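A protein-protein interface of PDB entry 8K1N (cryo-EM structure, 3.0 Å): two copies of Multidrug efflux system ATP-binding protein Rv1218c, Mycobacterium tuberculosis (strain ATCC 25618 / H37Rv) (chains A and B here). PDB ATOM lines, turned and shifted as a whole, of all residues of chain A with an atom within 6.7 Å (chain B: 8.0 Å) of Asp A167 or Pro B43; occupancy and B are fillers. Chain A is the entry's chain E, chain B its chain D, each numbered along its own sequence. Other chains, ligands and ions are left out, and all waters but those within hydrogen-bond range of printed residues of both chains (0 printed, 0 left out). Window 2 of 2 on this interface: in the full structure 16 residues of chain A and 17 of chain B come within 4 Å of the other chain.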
ATOM      1  N   GLY A 139     -15.948  -5.783  -7.349  1.00  0.00           N
ATOM      2  CA  GLY A 139     -17.011  -6.752  -7.098  1.00  0.00           C
ATOM      3  C   GLY A 139     -16.417  -8.098  -6.895  1.00  0.00           C
ATOM      4  O   GLY A 139     -16.795  -8.663  -5.926  1.00  0.00           O
ATOM      5  N   LYS A 143     -15.841 -10.974  -3.225  1.00  0.00           N
ATOM      6  CA  LYS A 143     -16.261 -12.369  -3.269  1.00  0.00           C
ATOM      7  C   LYS A 143     -15.215 -13.290  -2.666  1.00  0.00           C
ATOM      8  O   LYS A 143     -15.565 -14.306  -2.065  1.00  0.00           O
ATOM      9  CB  LYS A 143     -16.561 -12.788  -4.705  1.00  0.00           C
ATOM     10  CG  LYS A 143     -17.750 -12.090  -5.324  1.00  0.00           C
ATOM     11  CD  LYS A 143     -17.974 -12.577  -6.740  1.00  0.00           C
ATOM     12  CE  LYS A 143     -18.976 -11.714  -7.472  1.00  0.00           C
ATOM     13  NZ  LYS A 143     -19.014 -12.038  -8.920  1.00  0.00           N
ATOM     14  N   GLY A 165     -19.681  -3.261  -3.171  1.00  0.00           N
ATOM     15  CA  GLY A 165     -19.349  -3.504  -4.555  1.00  0.00           C
ATOM     16  C   GLY A 165     -20.106  -4.637  -5.203  1.00  0.00           C
ATOM     17  O   GLY A 165     -19.758  -5.030  -6.320  1.00  0.00           O
ATOM     18  N   LEU A 166     -21.131  -5.168  -4.545  1.00  0.00           N
ATOM     19  CA  LEU A 166     -21.882  -6.312  -5.036  1.00  0.00           C
ATOM     20  C   LEU A 166     -23.206  -5.856  -5.631  1.00  0.00           C
ATOM     21  O   LEU A 166     -23.956  -5.110  -4.995  1.00  0.00           O
ATOM     22  CB  LEU A 166     -22.144  -7.309  -3.905  1.00  0.00           C
ATOM     23  CG  LEU A 166     -21.176  -8.480  -3.734  1.00  0.00           C
ATOM     24  CD1 LEU A 166     -19.770  -7.990  -3.499  1.00  0.00           C
ATOM     25  CD2 LEU A 166     -21.623  -9.354  -2.581  1.00  0.00           C
ATOM     26  N   ASP A 167     -23.465  -6.375  -6.835  1.00  0.00           N
ATOM     27  CA  ASP A 167     -24.736  -6.091  -7.534  1.00  0.00           C
ATOM     28  C   ASP A 167     -25.903  -6.681  -6.767  1.00  0.00           C
ATOM     29  O   ASP A 167     -25.687  -7.603  -5.951  1.00  0.00           O
ATOM     30  CB  ASP A 167     -24.814  -6.815  -8.869  1.00  0.00           C
ATOM     31  CG  ASP A 167     -24.754  -8.329  -8.787  1.00  0.00           C
ATOM     32  OD1 ASP A 167     -24.572  -8.851  -7.671  1.00  0.00           O
ATOM     33  OD2 ASP A 167     -24.858  -8.970  -9.846  1.00  0.00           O
ATOM     34  N   PRO A 168     -27.147  -6.229  -7.013  1.00  0.00           N
ATOM     35  CA  PRO A 168     -28.273  -6.732  -6.204  1.00  0.00           C
ATOM     36  C   PRO A 168     -28.451  -8.238  -6.260  1.00  0.00           C
ATOM     37  O   PRO A 168     -28.952  -8.823  -5.290  1.00  0.00           O
ATOM     38  CB  PRO A 168     -29.481  -6.001  -6.804  1.00  0.00           C
ATOM     39  CG  PRO A 168     -28.916  -4.753  -7.356  1.00  0.00           C
ATOM     40  CD  PRO A 168     -27.569  -5.114  -7.885  1.00  0.00           C
ATOM     41  N   LEU A 169     -28.064  -8.893  -7.355  1.00  0.00           N
ATOM     42  CA  LEU A 169     -28.185 -10.347  -7.422  1.00  0.00           C
ATOM     43  C   LEU A 169     -27.244 -11.023  -6.430  1.00  0.00           C
ATOM     44  O   LEU A 169     -27.645 -11.936  -5.696  1.00  0.00           O
ATOM     45  CB  LEU A 169     -27.908 -10.828  -8.843  1.00  0.00           C
ATOM     46  CG  LEU A 169     -28.905 -10.380  -9.909  1.00  0.00           C
ATOM     47  CD1 LEU A 169     -28.432 -10.801 -11.283  1.00  0.00           C
ATOM     48  CD2 LEU A 169     -30.274 -10.953  -9.625  1.00  0.00           C
ATOM     49  N   MET A 170     -25.986 -10.581  -6.384  1.00  0.00           N
ATOM     50  CA  MET A 170     -25.060 -11.148  -5.413  1.00  0.00           C
ATOM     51  C   MET A 170     -25.411 -10.715  -3.998  1.00  0.00           C
ATOM     52  O   MET A 170     -25.140 -11.448  -3.045  1.00  0.00           O
ATOM     53  CB  MET A 170     -23.627 -10.765  -5.760  1.00  0.00           C
ATOM     54  CG  MET A 170     -23.171 -11.309  -7.098  1.00  0.00           C
ATOM     55  SD  MET A 170     -23.473 -13.074  -7.259  1.00  0.00           S
ATOM     56  CE  MET A 170     -22.996 -13.336  -8.962  1.00  0.00           C
ATOM     57  N   GLU A 171     -26.033  -9.548  -3.844  1.00  0.00           N
ATOM     58  CA  GLU A 171     -26.581  -9.166  -2.547  1.00  0.00           C
ATOM     59  C   GLU A 171     -27.632 -10.167  -2.085  1.00  0.00           C
ATOM     60  O   GLU A 171     -27.630 -10.600  -0.927  1.00  0.00           O
ATOM     61  CB  GLU A 171     -27.177  -7.763  -2.631  1.00  0.00           C
ATOM     62  CG  GLU A 171     -27.967  -7.349  -1.408  1.00  0.00           C
ATOM     63  CD  GLU A 171     -27.098  -7.141  -0.196  1.00  0.00           C
ATOM     64  OE1 GLU A 171     -25.912  -6.797  -0.373  1.00  0.00           O
ATOM     65  OE2 GLU A 171     -27.596  -7.320   0.934  1.00  0.00           O
ATOM     66  N   ASN A 172     -28.539 -10.551  -2.984  1.00  0.00           N
ATOM     67  CA  ASN A 172     -29.560 -11.531  -2.632  1.00  0.00           C
ATOM     68  C   ASN A 172     -28.939 -12.882  -2.304  1.00  0.00           C
ATOM     69  O   ASN A 172     -29.369 -13.560  -1.362  1.00  0.00           O
ATOM     70  CB  ASN A 172     -30.565 -11.667  -3.772  1.00  0.00           C
ATOM     71  CG  ASN A 172     -31.882 -12.249  -3.318  1.00  0.00           C
ATOM     72  OD1 ASN A 172     -32.527 -11.723  -2.415  1.00  0.00           O
ATOM     73  ND2 ASN A 172     -32.293 -13.342  -3.946  1.00  0.00           N
ATOM     74  N   PHE B  40     -29.672   2.971 -13.345  1.00  0.00           N
ATOM     75  CA  PHE B  40     -29.072   2.062 -14.318  1.00  0.00           C
ATOM     76  C   PHE B  40     -28.717   0.776 -13.578  1.00  0.00           C
ATOM     77  O   PHE B  40     -27.665   0.696 -12.938  1.00  0.00           O
ATOM     78  CB  PHE B  40     -27.853   2.718 -14.959  1.00  0.00           C
ATOM     79  CG  PHE B  40     -27.362   2.035 -16.197  1.00  0.00           C
ATOM     80  CD1 PHE B  40     -28.245   1.604 -17.164  1.00  0.00           C
ATOM     81  CD2 PHE B  40     -26.007   1.878 -16.420  1.00  0.00           C
ATOM     82  CE1 PHE B  40     -27.791   0.992 -18.308  1.00  0.00           C
ATOM     83  CE2 PHE B  40     -25.551   1.271 -17.564  1.00  0.00           C
ATOM     84  CZ  PHE B  40     -26.443   0.827 -18.509  1.00  0.00           C
ATOM     85  N   LEU B  41     -29.588  -0.228 -13.659  1.00  0.00           N
ATOM     86  CA  LEU B  41     -29.505  -1.406 -12.812  1.00  0.00           C
ATOM     87  C   LEU B  41     -29.148  -2.653 -13.615  1.00  0.00           C
ATOM     88  O   LEU B  41     -29.552  -2.812 -14.773  1.00  0.00           O
ATOM     89  CB  LEU B  41     -30.827  -1.638 -12.077  1.00  0.00           C
ATOM     90  CG  LEU B  41     -31.407  -0.441 -11.328  1.00  0.00           C
ATOM     91  CD1 LEU B  41     -32.867  -0.677 -11.013  1.00  0.00           C
ATOM     92  CD2 LEU B  41     -30.622  -0.190 -10.062  1.00  0.00           C
ATOM     93  N   GLY B  42     -28.397  -3.537 -12.970  1.00  0.00           N
ATOM     94  CA  GLY B  42     -27.991  -4.793 -13.550  1.00  0.00           C
ATOM     95  C   GLY B  42     -26.872  -5.428 -12.752  1.00  0.00           C
ATOM     96  O   GLY B  42     -26.295  -4.808 -11.855  1.00  0.00           O
ATOM     97  N   PRO B  43     -26.520  -6.696 -12.979  1.00  0.00           N
ATOM     98  CA  PRO B  43     -25.433  -7.256 -12.277  1.00  0.00           C
ATOM     99  C   PRO B  43     -24.072  -6.746 -12.728  1.00  0.00           C
ATOM    100  O   PRO B  43     -24.002  -5.937 -13.573  1.00  0.00           O
ATOM    101  CB  PRO B  43     -25.401  -8.650 -12.852  1.00  0.00           C
ATOM    102  CG  PRO B  43     -26.159  -8.622 -14.118  1.00  0.00           C
ATOM    103  CD  PRO B  43     -27.274  -7.697 -13.750  1.00  0.00           C
ATOM    104  N   ASN B  44     -23.007  -7.266 -12.115  1.00  0.00           N
ATOM    105  CA  ASN B  44     -21.674  -6.817 -12.498  1.00  0.00           C
ATOM    106  C   ASN B  44     -21.193  -7.106 -13.916  1.00  0.00           C
ATOM    107  O   ASN B  44     -20.529  -6.264 -14.530  1.00  0.00           O
ATOM    108  CB  ASN B  44     -20.682  -7.369 -11.478  1.00  0.00           C
ATOM    109  CG  ASN B  44     -20.444  -6.415 -10.328  1.00  0.00           C
ATOM    110  OD1 ASN B  44     -20.411  -5.202 -10.511  1.00  0.00           O
ATOM    111  ND2 ASN B  44     -20.272  -6.962  -9.132  1.00  0.00           N
ATOM    112  N   GLY B  45     -21.510  -8.278 -14.452  1.00  0.00           N
ATOM    113  CA  GLY B  45     -21.080  -8.642 -15.784  1.00  0.00           C
ATOM    114  C   GLY B  45     -22.039  -8.285 -16.896  1.00  0.00           C
ATOM    115  O   GLY B  45     -21.842  -8.732 -18.030  1.00  0.00           O
ATOM    116  N   ALA B  46     -23.069  -7.489 -16.617  1.00  0.00           N
ATOM    117  CA  ALA B  46     -24.101  -7.196 -17.600  1.00  0.00           C
ATOM    118  C   ALA B  46     -23.705  -6.112 -18.593  1.00  0.00           C
ATOM    119  O   ALA B  46     -24.397  -5.942 -19.601  1.00  0.00           O
ATOM    120  CB  ALA B  46     -25.392  -6.784 -16.893  1.00  0.00           C
ATOM    121  N   GLY B  47     -22.636  -5.374 -18.340  1.00  0.00           N
ATOM    122  CA  GLY B  47     -22.170  -4.361 -19.253  1.00  0.00           C
ATOM    123  C   GLY B  47     -22.477  -2.921 -18.887  1.00  0.00           C
ATOM    124  O   GLY B  47     -22.563  -2.082 -19.791  1.00  0.00           O
ATOM    125  N   LYS B  48     -22.662  -2.609 -17.604  1.00  0.00           N
ATOM    126  CA  LYS B  48     -22.814  -1.214 -17.205  1.00  0.00           C
ATOM    127  C   LYS B  48     -21.476  -0.489 -17.238  1.00  0.00           C
ATOM    128  O   LYS B  48     -21.393   0.663 -17.683  1.00  0.00           O
ATOM    129  CB  LYS B  48     -23.428  -1.130 -15.812  1.00  0.00           C
ATOM    130  CG  LYS B  48     -24.707  -1.919 -15.645  1.00  0.00           C
ATOM    131  CD  LYS B  48     -25.468  -1.456 -14.422  1.00  0.00           C
ATOM    132  CE  LYS B  48     -24.547  -1.294 -13.232  1.00  0.00           C
ATOM    133  NZ  LYS B  48     -25.296  -0.959 -11.996  1.00  0.00           N
ATOM    134  N   SER B  49     -20.419  -1.152 -16.766  1.00  0.00           N
ATOM    135  CA  SER B  49     -19.092  -0.554 -16.807  1.00  0.00           C
ATOM    136  C   SER B  49     -18.654  -0.301 -18.241  1.00  0.00           C
ATOM    137  O   SER B  49     -18.080   0.748 -18.543  1.00  0.00           O
ATOM    138  CB  SER B  49     -18.087  -1.452 -16.092  1.00  0.00           C
ATOM    139  OG  SER B  49     -16.838  -0.802 -15.955  1.00  0.00           O
ATOM    140  N   GLU B 161     -21.593   3.722  -8.440  1.00  0.00           N
ATOM    141  CA  GLU B 161     -21.530   3.392  -7.021  1.00  0.00           C
ATOM    142  C   GLU B 161     -21.067   4.612  -6.216  1.00  0.00           C
ATOM    143  O   GLU B 161     -20.022   4.570  -5.566  1.00  0.00           O
ATOM    144  CB  GLU B 161     -20.613   2.203  -6.772  1.00  0.00           C
ATOM    145  CG  GLU B 161     -20.950   0.988  -7.607  1.00  0.00           C
ATOM    146  CD  GLU B 161     -20.087  -0.205  -7.262  1.00  0.00           C
ATOM    147  OE1 GLU B 161     -19.930  -0.499  -6.059  1.00  0.00           O
ATOM    148  OE2 GLU B 161     -19.564  -0.850  -8.194  1.00  0.00           O
ATOM    149  N   SER B 192     -26.215   2.384  -9.316  1.00  0.00           N
ATOM    150  CA  SER B 192     -26.007   2.344  -7.871  1.00  0.00           C
ATOM    151  C   SER B 192     -25.492   1.006  -7.338  1.00  0.00           C
ATOM    152  O   SER B 192     -24.439   0.966  -6.692  1.00  0.00           O
ATOM    153  CB  SER B 192     -27.311   2.720  -7.164  1.00  0.00           C
ATOM    154  OG  SER B 192     -27.158   2.647  -5.760  1.00  0.00           O
ATOM    155  N   HIS B 193     -26.224  -0.084  -7.580  1.00  0.00           N
ATOM    156  CA  HIS B 193     -26.147  -1.398  -6.908  1.00  0.00           C
ATOM    157  C   HIS B 193     -26.815  -1.402  -5.537  1.00  0.00           C
ATOM    158  O   HIS B 193     -26.836  -2.452  -4.893  1.00  0.00           O
ATOM    159  CB  HIS B 193     -24.724  -1.956  -6.709  1.00  0.00           C
ATOM    160  CG  HIS B 193     -23.957  -2.167  -7.976  1.00  0.00           C
ATOM    161  ND1 HIS B 193     -24.291  -3.143  -8.888  1.00  0.00           N
ATOM    162  CD2 HIS B 193     -22.855  -1.557  -8.464  1.00  0.00           C
ATOM    163  CE1 HIS B 193     -23.439  -3.111  -9.896  1.00  0.00           C
ATOM    164  NE2 HIS B 193     -22.557  -2.156  -9.664  1.00  0.00           N
ATOM    165  N   ILE B 194     -27.351  -0.282  -5.069  1.00  0.00           N
ATOM    166  CA  ILE B 194     -28.078  -0.222  -3.805  1.00  0.00           C
ATOM    167  C   ILE B 194     -29.466   0.305  -4.138  1.00  0.00           C
ATOM    168  O   ILE B 194     -29.642   1.502  -4.393  1.00  0.00           O
ATOM    169  CB  ILE B 194     -27.377   0.658  -2.768  1.00  0.00           C
ATOM    170  CG1 ILE B 194     -26.016   0.067  -2.411  1.00  0.00           C
ATOM    171  CG2 ILE B 194     -28.231   0.793  -1.526  1.00  0.00           C
ATOM    172  CD1 ILE B 194     -25.331   0.775  -1.275  1.00  0.00           C
ATOM    173  N   LEU B 195     -30.458  -0.583  -4.135  1.00  0.00           N
ATOM    174  CA  LEU B 195     -31.775  -0.221  -4.642  1.00  0.00           C
ATOM    175  C   LEU B 195     -32.534   0.710  -3.705  1.00  0.00           C
ATOM    176  O   LEU B 195     -33.499   1.344  -4.138  1.00  0.00           O
ATOM    177  CB  LEU B 195     -32.587  -1.485  -4.914  1.00  0.00           C
ATOM    178  CG  LEU B 195     -31.806  -2.598  -5.615  1.00  0.00           C
ATOM    179  CD1 LEU B 195     -32.629  -3.866  -5.702  1.00  0.00           C
ATOM    180  CD2 LEU B 195     -31.364  -2.156  -6.994  1.00  0.00           C
ATOM    181  N   ILE B 207     -33.281  -1.617 -16.429  1.00  0.00           N
ATOM    182  CA  ILE B 207     -32.674  -2.853 -15.946  1.00  0.00           C
ATOM    183  C   ILE B 207     -32.183  -3.652 -17.143  1.00  0.00           C
ATOM    184  O   ILE B 207     -32.960  -3.938 -18.068  1.00  0.00           O
ATOM    185  CB  ILE B 207     -33.674  -3.681 -15.122  1.00  0.00           C
ATOM    186  CG1 ILE B 207     -34.347  -2.814 -14.062  1.00  0.00           C
ATOM    187  CG2 ILE B 207     -32.983  -4.868 -14.485  1.00  0.00           C
ATOM    188  CD1 ILE B 207     -35.655  -3.373 -13.573  1.00  0.00           C
ATOM    189  N   ILE B 208     -30.904  -4.038 -17.107  1.00  0.00           N
ATOM    190  CA  ILE B 208     -30.250  -4.770 -18.187  1.00  0.00           C
ATOM    191  C   ILE B 208     -29.770  -6.117 -17.658  1.00  0.00           C
ATOM    192  O   ILE B 208     -29.339  -6.222 -16.506  1.00  0.00           O
ATOM    193  CB  ILE B 208     -29.078  -3.962 -18.787  1.00  0.00           C
ATOM    194  CG1 ILE B 208     -27.839  -4.032 -17.899  1.00  0.00           C
ATOM    195  CG2 ILE B 208     -29.474  -2.516 -18.982  1.00  0.00           C
ATOM    196  CD1 ILE B 208     -26.629  -3.402 -18.519  1.00  0.00           C
ATOM    197  N   ARG B 209     -29.888  -7.164 -18.484  1.00  0.00           N
ATOM    198  CA  ARG B 209     -29.525  -8.511 -18.047  1.00  0.00           C
ATOM    199  C   ARG B 209     -28.172  -8.979 -18.576  1.00  0.00           C
ATOM    200  O   ARG B 209     -27.261  -9.248 -17.788  1.00  0.00           O
ATOM    201  CB  ARG B 209     -30.610  -9.514 -18.456  1.00  0.00           C
ATOM    202  CG  ARG B 209     -30.543 -10.827 -17.690  1.00  0.00           C
ATOM    203  CD  ARG B 209     -31.448 -11.883 -18.295  1.00  0.00           C
ATOM    204  NE  ARG B 209     -32.860 -11.563 -18.108  1.00  0.00           N
ATOM    205  CZ  ARG B 209     -33.834 -11.991 -18.904  1.00  0.00           C
ATOM    206  NH1 ARG B 209     -35.091 -11.652 -18.660  1.00  0.00           N
ATOM    207  NH2 ARG B 209     -33.548 -12.757 -19.947  1.00  0.00           N
ATOM    208  N   ALA B 210     -28.018  -9.093 -19.895  1.00  0.00           N
ATOM    209  CA  ALA B 210     -26.771  -9.605 -20.457  1.00  0.00           C
ATOM    210  C   ALA B 210     -26.063  -8.575 -21.326  1.00  0.00           C
ATOM    211  O   ALA B 210     -24.925  -8.203 -21.030  1.00  0.00           O
ATOM    212  CB  ALA B 210     -27.046 -10.883 -21.256  1.00  0.00           C
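Printed residues of chain A that touch a printed residue of chain B: Gly A139, Gly A165, Leu A166, Asp A167 and Pro A168. Hydrophobic or aromatic side chains of chain A that line the printed part of chain B: Pro A168. Among the printed residues, no Asp or Glu carboxylate lies within 4 Å of a Lys or Arg side-chain nitrogen of the other chain.
The side-chain carboxylate (OD2) of Asp A167 sits at hydrogen-bond distance from the backbone NH (N) of Asn B44 (3.4 Å). The side-chain amide nitrogen of Asn B44 sits at hydrogen-bond distance from the backbone carbonyl oxygen of Gly A165 (3.5 Å).
No position is printed for both chains.
Printed residues of chain B within 4 Å of Gly A139: Asn B44. Of the printed residues of chain B, Gly A165 touches Asn B44 (3.5 Å) and Glu B161 (3.4 Å). Of chain B, only Gly B42 (3.9 Å), Pro B43 (3.0 Å), Asn B44 (3.4 Å) and His B193 (3.3 Å) come within 4 Å of Asp A167. Of chain B, only His B193 and Leu B195 come within 4 Å of Pro A168. Of the printed residues of chain A, Gly B42 touches Asp A167. Pro B43 touches one residue of chain A. Printed residues of chain A within 4 Å of Asn B44: Gly A139 (3.8 Å), Gly A165 (3.5 Å) and Asp A167 (3.4 Å). Printed residues of chain A within 4 Å of Leu B195: Pro A168. Ala B210 touches none of the printed residues of chain A.
The side-chain carboxylate (OD1) of Asp A167 lies within hydrogen-bond range of the backbone NH (N) of Met A170 (2.6 Å).
Gly A139 touches Asn B44. Gly A165 touches Glu B161 (CA to OE1, 3.4 Å). O of Leu A166 touches CB of His B193, at 3.7 Å. CB of Asp A167 touches O of Gly B42, at 3.9 Å. OD2 of Asp A167 touches CA of Pro B43, at 3.0 Å. His B193 touches Asp A167 (ND1 to CA, 3.3 Å). Pro A168 touches His B193 (CD to ND1, 3.95 Å). Pro A168 touches Leu B195.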
